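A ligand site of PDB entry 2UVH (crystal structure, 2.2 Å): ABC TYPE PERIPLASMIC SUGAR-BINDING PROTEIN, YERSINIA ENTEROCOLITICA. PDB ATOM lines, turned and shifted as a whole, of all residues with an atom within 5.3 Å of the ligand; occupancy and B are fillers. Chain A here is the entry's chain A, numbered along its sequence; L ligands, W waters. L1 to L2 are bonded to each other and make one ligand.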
ATOM      1  N   TRP A  13     -23.811  11.989  17.671  1.00  0.00           N
ATOM      2  CA  TRP A  13     -23.319  10.764  18.328  1.00  0.00           C
ATOM      3  C   TRP A  13     -24.492   9.883  18.777  1.00  0.00           C
ATOM      4  O   TRP A  13     -25.635  10.333  18.823  1.00  0.00           O
ATOM      5  CB  TRP A  13     -22.401  11.098  19.531  1.00  0.00           C
ATOM      6  CG  TRP A  13     -23.202  11.483  20.727  1.00  0.00           C
ATOM      7  CD1 TRP A  13     -23.707  10.628  21.698  1.00  0.00           C
ATOM      8  CD2 TRP A  13     -23.604  12.813  21.110  1.00  0.00           C
ATOM      9  NE1 TRP A  13     -24.435  11.354  22.614  1.00  0.00           N
ATOM     10  CE2 TRP A  13     -24.379  12.692  22.288  1.00  0.00           C
ATOM     11  CE3 TRP A  13     -23.413  14.099  20.545  1.00  0.00           C
ATOM     12  CZ2 TRP A  13     -24.939  13.815  22.922  1.00  0.00           C
ATOM     13  CZ3 TRP A  13     -23.976  15.206  21.193  1.00  0.00           C
ATOM     14  CH2 TRP A  13     -24.722  15.058  22.347  1.00  0.00           C
ATOM     15  N   GLY A  14     -24.225   8.624  19.104  1.00  0.00           N
ATOM     16  CA  GLY A  14     -25.193   7.721  19.743  1.00  0.00           C
ATOM     17  C   GLY A  14     -24.900   6.248  19.375  1.00  0.00           C
ATOM     18  O   GLY A  14     -23.896   5.962  18.742  1.00  0.00           O
ATOM     19  N   ARG A  18     -29.863   4.683  17.139  1.00  0.00           N
ATOM     20  CA  ARG A  18     -29.975   6.136  16.860  1.00  0.00           C
ATOM     21  C   ARG A  18     -29.393   6.487  15.523  1.00  0.00           C
ATOM     22  O   ARG A  18     -29.975   7.265  14.793  1.00  0.00           O
ATOM     23  CB  ARG A  18     -29.378   6.998  17.988  1.00  0.00           C
ATOM     24  CG  ARG A  18     -29.299   8.504  17.649  1.00  0.00           C
ATOM     25  CD  ARG A  18     -28.625   9.268  18.742  1.00  0.00           C
ATOM     26  NE  ARG A  18     -29.335   9.111  20.005  1.00  0.00           N
ATOM     27  CZ  ARG A  18     -28.829   9.435  21.184  1.00  0.00           C
ATOM     28  NH1 ARG A  18     -27.588   9.946  21.251  1.00  0.00           N
ATOM     29  NH2 ARG A  18     -29.529   9.253  22.289  1.00  0.00           N
ATOM     30  N   TRP A  45     -20.505   8.194  21.465  1.00  0.00           N
ATOM     31  CA  TRP A  45     -20.106   9.281  22.351  1.00  0.00           C
ATOM     32  C   TRP A  45     -18.586   9.463  22.460  1.00  0.00           C
ATOM     33  O   TRP A  45     -18.081  10.592  22.378  1.00  0.00           O
ATOM     34  CB  TRP A  45     -20.635   9.034  23.767  1.00  0.00           C
ATOM     35  CG  TRP A  45     -20.163  10.055  24.767  1.00  0.00           C
ATOM     36  CD1 TRP A  45     -19.314   9.838  25.828  1.00  0.00           C
ATOM     37  CD2 TRP A  45     -20.514  11.440  24.794  1.00  0.00           C
ATOM     38  NE1 TRP A  45     -19.100  11.040  26.519  1.00  0.00           N
ATOM     39  CE2 TRP A  45     -19.840  12.030  25.898  1.00  0.00           C
ATOM     40  CE3 TRP A  45     -21.353  12.261  23.999  1.00  0.00           C
ATOM     41  CZ2 TRP A  45     -19.983  13.377  26.229  1.00  0.00           C
ATOM     42  CZ3 TRP A  45     -21.481  13.607  24.317  1.00  0.00           C
ATOM     43  CH2 TRP A  45     -20.804  14.156  25.431  1.00  0.00           C
ATOM     44  N   ASN A  68     -24.198  19.035  23.180  1.00  0.00           N
ATOM     45  CA  ASN A  68     -24.465  18.765  24.553  1.00  0.00           C
ATOM     46  C   ASN A  68     -24.528  20.077  25.288  1.00  0.00           C
ATOM     47  O   ASN A  68     -23.870  21.057  24.940  1.00  0.00           O
ATOM     48  CB  ASN A  68     -23.413  17.808  25.154  1.00  0.00           C
ATOM     49  CG  ASN A  68     -24.028  16.681  25.954  1.00  0.00           C
ATOM     50  OD1 ASN A  68     -25.216  16.345  25.797  1.00  0.00           O
ATOM     51  ND2 ASN A  68     -23.233  16.086  26.850  1.00  0.00           N
ATOM     52  N   THR A 119     -33.575  15.071  30.575  1.00  0.00           N
ATOM     53  CA  THR A 119     -33.093  13.837  31.142  1.00  0.00           C
ATOM     54  C   THR A 119     -32.498  14.077  32.536  1.00  0.00           C
ATOM     55  O   THR A 119     -32.091  15.180  32.877  1.00  0.00           O
ATOM     56  CB  THR A 119     -32.067  13.151  30.154  1.00  0.00           C
ATOM     57  OG1 THR A 119     -31.882  11.779  30.525  1.00  0.00           O
ATOM     58  CG2 THR A 119     -30.695  13.904  30.091  1.00  0.00           C
ATOM     59  N   ARG A 121     -29.994  11.516  35.361  1.00  0.00           N
ATOM     60  CA  ARG A 121     -29.509  10.145  35.669  1.00  0.00           C
ATOM     61  C   ARG A 121     -30.365   9.544  36.775  1.00  0.00           C
ATOM     62  O   ARG A 121     -30.520  10.157  37.803  1.00  0.00           O
ATOM     63  CB  ARG A 121     -28.043  10.109  36.124  1.00  0.00           C
ATOM     64  CG  ARG A 121     -27.017  10.526  35.093  1.00  0.00           C
ATOM     65  CD  ARG A 121     -25.604  10.231  35.572  1.00  0.00           C
ATOM     66  NE  ARG A 121     -24.598  10.607  34.587  1.00  0.00           N
ATOM     67  CZ  ARG A 121     -24.172   9.840  33.595  1.00  0.00           C
ATOM     68  NH1 ARG A 121     -24.642   8.596  33.451  1.00  0.00           N
ATOM     69  NH2 ARG A 121     -23.262  10.296  32.764  1.00  0.00           N
ATOM     70  N   GLU A 165     -19.499   4.062  35.750  1.00  0.00           N
ATOM     71  CA  GLU A 165     -18.314   4.653  35.122  1.00  0.00           C
ATOM     72  C   GLU A 165     -18.058   5.881  35.923  1.00  0.00           C
ATOM     73  O   GLU A 165     -18.948   6.306  36.706  1.00  0.00           O
ATOM     74  CB  GLU A 165     -18.564   5.012  33.676  1.00  0.00           C
ATOM     75  CG  GLU A 165     -18.918   3.796  32.881  1.00  0.00           C
ATOM     76  CD  GLU A 165     -19.269   4.155  31.438  1.00  0.00           C
ATOM     77  OE1 GLU A 165     -18.347   4.327  30.619  1.00  0.00           O
ATOM     78  OE2 GLU A 165     -20.470   4.255  31.136  1.00  0.00           O
ATOM     79  N   GLN A 167     -17.845   9.123  35.480  1.00  0.00           N
ATOM     80  CA  GLN A 167     -18.786  10.230  35.355  1.00  0.00           C
ATOM     81  C   GLN A 167     -20.140   9.982  36.089  1.00  0.00           C
ATOM     82  O   GLN A 167     -20.732  10.921  36.680  1.00  0.00           O
ATOM     83  CB  GLN A 167     -19.004  10.526  33.878  1.00  0.00           C
ATOM     84  CG  GLN A 167     -19.843  11.764  33.588  1.00  0.00           C
ATOM     85  CD  GLN A 167     -20.070  11.949  32.118  1.00  0.00           C
ATOM     86  OE1 GLN A 167     -20.154  10.990  31.373  1.00  0.00           O
ATOM     87  NE2 GLN A 167     -20.177  13.190  31.688  1.00  0.00           N
ATOM     88  N   ASP A 168     -20.625   8.731  36.039  1.00  0.00           N
ATOM     89  CA  ASP A 168     -21.845   8.301  36.743  1.00  0.00           C
ATOM     90  C   ASP A 168     -21.685   8.437  38.241  1.00  0.00           C
ATOM     91  O   ASP A 168     -22.546   8.988  38.913  1.00  0.00           O
ATOM     92  CB  ASP A 168     -22.179   6.842  36.498  1.00  0.00           C
ATOM     93  CG  ASP A 168     -22.138   6.456  35.060  1.00  0.00           C
ATOM     94  OD1 ASP A 168     -22.111   5.241  34.836  1.00  0.00           O
ATOM     95  OD2 ASP A 168     -22.139   7.346  34.165  1.00  0.00           O
ATOM     96  N   TYR A 231     -21.742  -0.828  27.832  1.00  0.00           N
ATOM     97  CA  TYR A 231     -22.929  -1.613  27.476  1.00  0.00           C
ATOM     98  C   TYR A 231     -22.601  -2.774  26.505  1.00  0.00           C
ATOM     99  O   TYR A 231     -23.472  -3.567  26.108  1.00  0.00           O
ATOM    100  CB  TYR A 231     -24.019  -0.687  26.899  1.00  0.00           C
ATOM    101  CG  TYR A 231     -23.496   0.277  25.886  1.00  0.00           C
ATOM    102  CD1 TYR A 231     -23.543  -0.027  24.503  1.00  0.00           C
ATOM    103  CD2 TYR A 231     -22.934   1.483  26.272  1.00  0.00           C
ATOM    104  CE1 TYR A 231     -23.041   0.867  23.569  1.00  0.00           C
ATOM    105  CE2 TYR A 231     -22.420   2.359  25.340  1.00  0.00           C
ATOM    106  CZ  TYR A 231     -22.481   2.053  23.987  1.00  0.00           C
ATOM    107  OH  TYR A 231     -21.966   2.950  23.054  1.00  0.00           O
ATOM    108  N   MET A 246     -28.115   6.151  35.063  1.00  0.00           N
ATOM    109  CA  MET A 246     -28.124   6.480  33.645  1.00  0.00           C
ATOM    110  C   MET A 246     -29.235   7.423  33.197  1.00  0.00           C
ATOM    111  O   MET A 246     -30.340   7.388  33.743  1.00  0.00           O
ATOM    112  CB  MET A 246     -28.169   5.166  32.814  1.00  0.00           C
ATOM    113  CG  MET A 246     -27.947   5.369  31.315  1.00  0.00           C
ATOM    114  SD  MET A 246     -26.448   6.230  30.869  1.00  0.00           S
ATOM    115  CE  MET A 246     -25.244   5.173  31.716  1.00  0.00           C
ATOM    116  N   TRP A 247     -28.884   8.279  32.260  1.00  0.00           N
ATOM    117  CA  TRP A 247     -29.818   9.121  31.538  1.00  0.00           C
ATOM    118  C   TRP A 247     -30.977   8.297  31.001  1.00  0.00           C
ATOM    119  O   TRP A 247     -30.782   7.359  30.229  1.00  0.00           O
ATOM    120  CB  TRP A 247     -29.096   9.743  30.329  1.00  0.00           C
ATOM    121  CG  TRP A 247     -27.839  10.486  30.680  1.00  0.00           C
ATOM    122  CD1 TRP A 247     -26.553  10.196  30.262  1.00  0.00           C
ATOM    123  CD2 TRP A 247     -27.749  11.617  31.531  1.00  0.00           C
ATOM    124  NE1 TRP A 247     -25.675  11.119  30.821  1.00  0.00           N
ATOM    125  CE2 TRP A 247     -26.379  11.993  31.602  1.00  0.00           C
ATOM    126  CE3 TRP A 247     -28.689  12.358  32.269  1.00  0.00           C
ATOM    127  CZ2 TRP A 247     -25.941  13.077  32.409  1.00  0.00           C
ATOM    128  CZ3 TRP A 247     -28.255  13.436  33.039  1.00  0.00           C
ATOM    129  CH2 TRP A 247     -26.891  13.776  33.109  1.00  0.00           C
ATOM    130  N   SER A 249     -32.884   9.158  28.844  1.00  0.00           N
ATOM    131  CA  SER A 249     -32.993   9.505  27.444  1.00  0.00           C
ATOM    132  C   SER A 249     -32.140   8.573  26.552  1.00  0.00           C
ATOM    133  O   SER A 249     -32.348   8.519  25.315  1.00  0.00           O
ATOM    134  CB  SER A 249     -32.549  10.942  27.257  1.00  0.00           C
ATOM    135  OG  SER A 249     -31.154  11.040  27.370  1.00  0.00           O
ATOM    136  N   THR A 250     -31.223   7.833  27.161  1.00  0.00           N
ATOM    137  CA  THR A 250     -30.399   6.889  26.409  1.00  0.00           C
ATOM    138  C   THR A 250     -30.376   5.500  27.028  1.00  0.00           C
ATOM    139  O   THR A 250     -29.422   4.742  26.848  1.00  0.00           O
ATOM    140  CB  THR A 250     -28.956   7.499  26.060  1.00  0.00           C
ATOM    141  OG1 THR A 250     -28.258   6.663  25.139  1.00  0.00           O
ATOM    142  CG2 THR A 250     -28.105   7.782  27.284  1.00  0.00           C
ATOM    143  N   LYS A 253     -29.785   2.191  24.825  1.00  0.00           N
ATOM    144  CA  LYS A 253     -28.428   1.851  24.406  1.00  0.00           C
ATOM    145  C   LYS A 253     -27.888   0.732  25.325  1.00  0.00           C
ATOM    146  O   LYS A 253     -26.932   0.009  24.969  1.00  0.00           O
ATOM    147  CB  LYS A 253     -27.536   3.108  24.474  1.00  0.00           C
ATOM    148  CG  LYS A 253     -26.117   2.932  23.963  1.00  0.00           C
ATOM    149  CD  LYS A 253     -25.382   4.262  23.703  1.00  0.00           C
ATOM    150  CE  LYS A 253     -24.870   4.902  24.982  1.00  0.00           C
ATOM    151  NZ  LYS A 253     -23.976   6.115  24.775  1.00  0.00           N
ATOM    152  N   TYR A 254     -28.504   0.586  26.512  1.00  0.00           N
ATOM    153  CA  TYR A 254     -28.017  -0.253  27.608  1.00  0.00           C
ATOM    154  C   TYR A 254     -28.811  -1.565  27.715  1.00  0.00           C
ATOM    155  O   TYR A 254     -28.234  -2.689  27.623  1.00  0.00           O
ATOM    156  CB  TYR A 254     -28.008   0.553  28.932  1.00  0.00           C
ATOM    157  CG  TYR A 254     -26.970   1.648  28.885  1.00  0.00           C
ATOM    158  CD1 TYR A 254     -25.678   1.401  29.336  1.00  0.00           C
ATOM    159  CD2 TYR A 254     -27.256   2.889  28.302  1.00  0.00           C
ATOM    160  CE1 TYR A 254     -24.717   2.369  29.248  1.00  0.00           C
ATOM    161  CE2 TYR A 254     -26.255   3.871  28.197  1.00  0.00           C
ATOM    162  CZ  TYR A 254     -24.982   3.586  28.677  1.00  0.00           C
ATOM    163  OH  TYR A 254     -23.974   4.538  28.601  1.00  0.00           O
ATOM    164  N   LYS A 283     -31.138  18.118  33.108  1.00  0.00           N
ATOM    165  CA  LYS A 283     -30.613  19.015  32.092  1.00  0.00           C
ATOM    166  C   LYS A 283     -31.323  18.671  30.781  1.00  0.00           C
ATOM    167  O   LYS A 283     -32.056  17.650  30.727  1.00  0.00           O
ATOM    168  CB  LYS A 283     -29.100  18.810  31.968  1.00  0.00           C
ATOM    169  CG  LYS A 283     -28.748  17.394  31.569  1.00  0.00           C
ATOM    170  CD  LYS A 283     -27.281  17.221  31.163  1.00  0.00           C
ATOM    171  CE  LYS A 283     -27.071  15.870  30.487  1.00  0.00           C
ATOM    172  NZ  LYS A 283     -25.610  15.525  30.353  1.00  0.00           N
ATOM    173  N   PRO A 284     -31.151  19.553  29.749  1.00  0.00           N
ATOM    174  CA  PRO A 284     -31.452  19.157  28.372  1.00  0.00           C
ATOM    175  C   PRO A 284     -30.505  18.044  27.953  1.00  0.00           C
ATOM    176  O   PRO A 284     -29.272  18.108  28.205  1.00  0.00           O
ATOM    177  CB  PRO A 284     -31.190  20.444  27.546  1.00  0.00           C
ATOM    178  CG  PRO A 284     -31.366  21.602  28.576  1.00  0.00           C
ATOM    179  CD  PRO A 284     -30.772  20.990  29.847  1.00  0.00           C
ATOM    180  N   ALA A 285     -31.065  17.023  27.304  1.00  0.00           N
ATOM    181  CA  ALA A 285     -30.320  15.794  27.085  1.00  0.00           C
ATOM    182  C   ALA A 285     -29.305  16.058  25.970  1.00  0.00           C
ATOM    183  O   ALA A 285     -28.158  15.585  25.996  1.00  0.00           O
ATOM    184  CB  ALA A 285     -31.268  14.698  26.704  1.00  0.00           C
ATOM    185  N   GLN A 286     -29.772  16.863  25.013  1.00  0.00           N
ATOM    186  CA  GLN A 286     -29.054  17.215  23.778  1.00  0.00           C
ATOM    187  C   GLN A 286     -29.841  18.260  22.981  1.00  0.00           C
ATOM    188  O   GLN A 286     -31.058  18.500  23.174  1.00  0.00           O
ATOM    189  CB  GLN A 286     -28.737  15.975  22.915  1.00  0.00           C
ATOM    190  CG  GLN A 286     -29.810  14.915  22.835  1.00  0.00           C
ATOM    191  CD  GLN A 286     -29.359  13.773  22.041  1.00  0.00           C
ATOM    192  OE1 GLN A 286     -28.785  12.812  22.567  1.00  0.00           O
ATOM    193  NE2 GLN A 286     -29.559  13.837  20.763  1.00  0.00           N
ATOM    194  N   ASP A 366     -20.106  19.439  34.764  1.00  0.00           N
ATOM    195  CA  ASP A 366     -19.835  18.489  33.644  1.00  0.00           C
ATOM    196  C   ASP A 366     -18.745  18.966  32.665  1.00  0.00           C
ATOM    197  O   ASP A 366     -18.784  18.646  31.467  1.00  0.00           O
ATOM    198  CB  ASP A 366     -21.130  18.166  32.897  1.00  0.00           C
ATOM    199  CG  ASP A 366     -21.115  16.831  32.237  1.00  0.00           C
ATOM    200  OD1 ASP A 366     -20.507  15.909  32.782  1.00  0.00           O
ATOM    201  OD2 ASP A 366     -21.779  16.634  31.178  1.00  0.00           O
HETATM  202  C1  LIG L   1     -23.721   8.503  29.327  1.00  0.00           C
HETATM  203  C2  LIG L   1     -24.030   8.235  27.842  1.00  0.00           C
HETATM  204  C3  LIG L   1     -23.093   8.993  26.920  1.00  0.00           C
HETATM  205  C4  LIG L   1     -22.739  10.380  27.421  1.00  0.00           C
HETATM  206  C5  LIG L   1     -22.152  10.334  28.833  1.00  0.00           C
HETATM  207  C6  LIG L   1     -22.060  11.782  29.260  1.00  0.00           C
HETATM  208  O1  LIG L   1     -22.833   7.546  29.792  1.00  0.00           O
HETATM  209  O2  LIG L   1     -23.954   6.836  27.532  1.00  0.00           O
HETATM  210  O3  LIG L   1     -23.657   9.084  25.623  1.00  0.00           O
HETATM  211  O4  LIG L   1     -23.904  11.201  27.557  1.00  0.00           O
HETATM  212  O5  LIG L   1     -23.098   9.731  29.704  1.00  0.00           O
HETATM  213  O6  LIG L   1     -22.880  12.102  30.095  1.00  0.00           O
HETATM  214  O7  LIG L   1     -21.252  12.612  28.770  1.00  0.00           O
HETATM  215  C1  LG2 L   2     -24.515  12.178  26.510  1.00  0.00           C
HETATM  216  C2  LG2 L   2     -25.297  13.286  27.130  1.00  0.00           C
HETATM  217  C3  LG2 L   2     -26.695  12.833  27.604  1.00  0.00           C
HETATM  218  C4  LG2 L   2     -27.414  12.197  26.421  1.00  0.00           C
HETATM  219  C5  LG2 L   2     -26.580  11.017  25.938  1.00  0.00           C
HETATM  220  C6  LG2 L   2     -27.238  10.311  24.791  1.00  0.00           C
HETATM  221  O1  LG2 L   2     -24.490  13.907  28.107  1.00  0.00           O
HETATM  222  O2  LG2 L   2     -27.385  13.966  28.078  1.00  0.00           O
HETATM  223  O3  LG2 L   2     -27.586  13.115  25.330  1.00  0.00           O
HETATM  224  O4  LG2 L   2     -25.200  11.330  25.588  1.00  0.00           O
HETATM  225  O5  LG2 L   2     -26.491   9.824  23.924  1.00  0.00           O
HETATM  226  O6  LG2 L   2     -28.472  10.171  24.770  1.00  0.00           O
HETATM  227  O   HOH W   1     -23.481  14.570  31.752  1.00  0.00           O
HETATM  228  O   HOH W   2     -25.441   7.389  23.327  1.00  0.00           O
HETATM  229  O   HOH W   3     -20.774  15.132  28.853  1.00  0.00           O
HETATM  230  O   HOH W   4     -18.069  11.492  29.230  1.00  0.00           O
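Water W3 lies within hydrogen-bond range of an oxygen (O7) of LIG L1 (2.6 Å), the side-chain carboxylate of Asp 366 (2.9 Å), the side-chain amide nitrogen of Asn 68 (3.3 Å) and the side-chain amide nitrogen of Gln 167 (3.5 Å).
Water W2 lies within hydrogen-bond range of the side-chain amino group of Lys 253 (2.4 Å), an oxygen (O5) of LG2 L2 (2.7 Å) and the side-chain hydroxyl of Thr 250 (3.4 Å).
Water W1 lies within hydrogen-bond range of the side-chain amino group (NZ) of Lys 283, the side-chain carboxylate (OD2) of Asp 366 and an oxygen (O6) of LIG L1.
Water W4 lies within hydrogen-bond range of the indole nitrogen (NE1) of Trp 45 (2.9 Å), the side-chain amide oxygen (OE1) of Gln 167 (3.0 Å) and an oxygen (O7) of LIG L1 (3.4 Å).
Merely in contact with the ligand: Thr 119 (3.9 Å), Met 246 (3.9 Å), Ser 249 (3.8 Å) and Thr 250 (3.0 Å).
Hydrophobic or aromatic side chains within 4 Å of the ligand: Trp 13, Trp 45, Met 246, Trp 247 and Tyr 254.
16 residues have an atom within 4 Å of the ligand: Trp 13, Arg 18, Trp 45, Asn 68, Thr 119, Arg 121, Gln 167, Met 246, Trp 247, Ser 249, Thr 250, Lys 253, Tyr 254, Lys 283, Ala 285 and Gln 286.
The nearest printed residue that does not touch the ligand is Glu 165 (4.3 Å).
The backbone NH of Ser 249 lies within hydrogen-bond range of the side-chain hydroxyl of Thr 119 (3.3 Å).
OE1 of Gln 167 is in hydrogen-bond range of NH2 of Arg 121 (3.5 Å).
The backbone carbonyl oxygen (O) of Lys 283 lies within hydrogen-bond range of the backbone NH (N) of Thr 119 (3.0 Å).
The side-chain amide oxygen (OD1) of Asn 68 lies close to the backbone carbonyl oxygen (O) of Ala 285 (3.0 Å).
NH1 of Arg 121 lies within salt-bridge range of OD2 of Asp 168 (2.9 Å).
The side-chain carboxylate (OD1) of Asp 366 sits at hydrogen-bond distance from the side-chain amide nitrogen (NE2) of Gln 167 (2.9 Å).
The guanidinium group of Arg 18 is in hydrogen-bond range of the side-chain amide oxygen of Gln 286, at 3.4 Å.
OH of Tyr 254 lies close to SD of Met 246 (3.8 Å).
An oxygen (O2) of LIG L1 lies within hydrogen-bond range of the side-chain hydroxyl (OH) of Tyr 254 (2.5 Å).
The guanidinium group (NH2) of Arg 121 is in salt-bridge range of an oxygen (O6) of LIG L1, at 3.2 Å.
The side-chain amino group of Lys 283 lies within hydrogen-bond range of an oxygen (O1) of LG2 L2 (3.0 Å).
O7 of LIG L1 lies close to NE1 of Trp 45, at 3.5 Å.
An oxygen (O5) of LG2 L2 sits at hydrogen-bond distance from the indole nitrogen (NE1) of Trp 13 (2.9 Å).
The guanidinium group of Arg 18 is in salt-bridge range of an oxygen (O6) of LG2 L2 (2.8 Å).
The indole nitrogen (NE1) of Trp 247 is in hydrogen-bond range of an oxygen (O6) of LIG L1, 3.1 Å away.
O3 of LG2 L2 is in hydrogen-bond range of OE1 of Gln 286 (3.0 Å).
The side-chain amino group of Lys 253 sits at hydrogen-bond distance from an oxygen (O2) of LIG L1 (2.8 Å).
An oxygen (O1) of LG2 L2 sits at hydrogen-bond distance from the side-chain amide nitrogen (ND2) of Asn 68, at 2.8 Å.
An oxygen (O3) of LG2 L2 sits at hydrogen-bond distance from the backbone carbonyl oxygen of Ala 285, 2.6 Å away.
NE2 of Gln 167 is in hydrogen-bond range of O7 of LIG L1 (3.2 Å).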
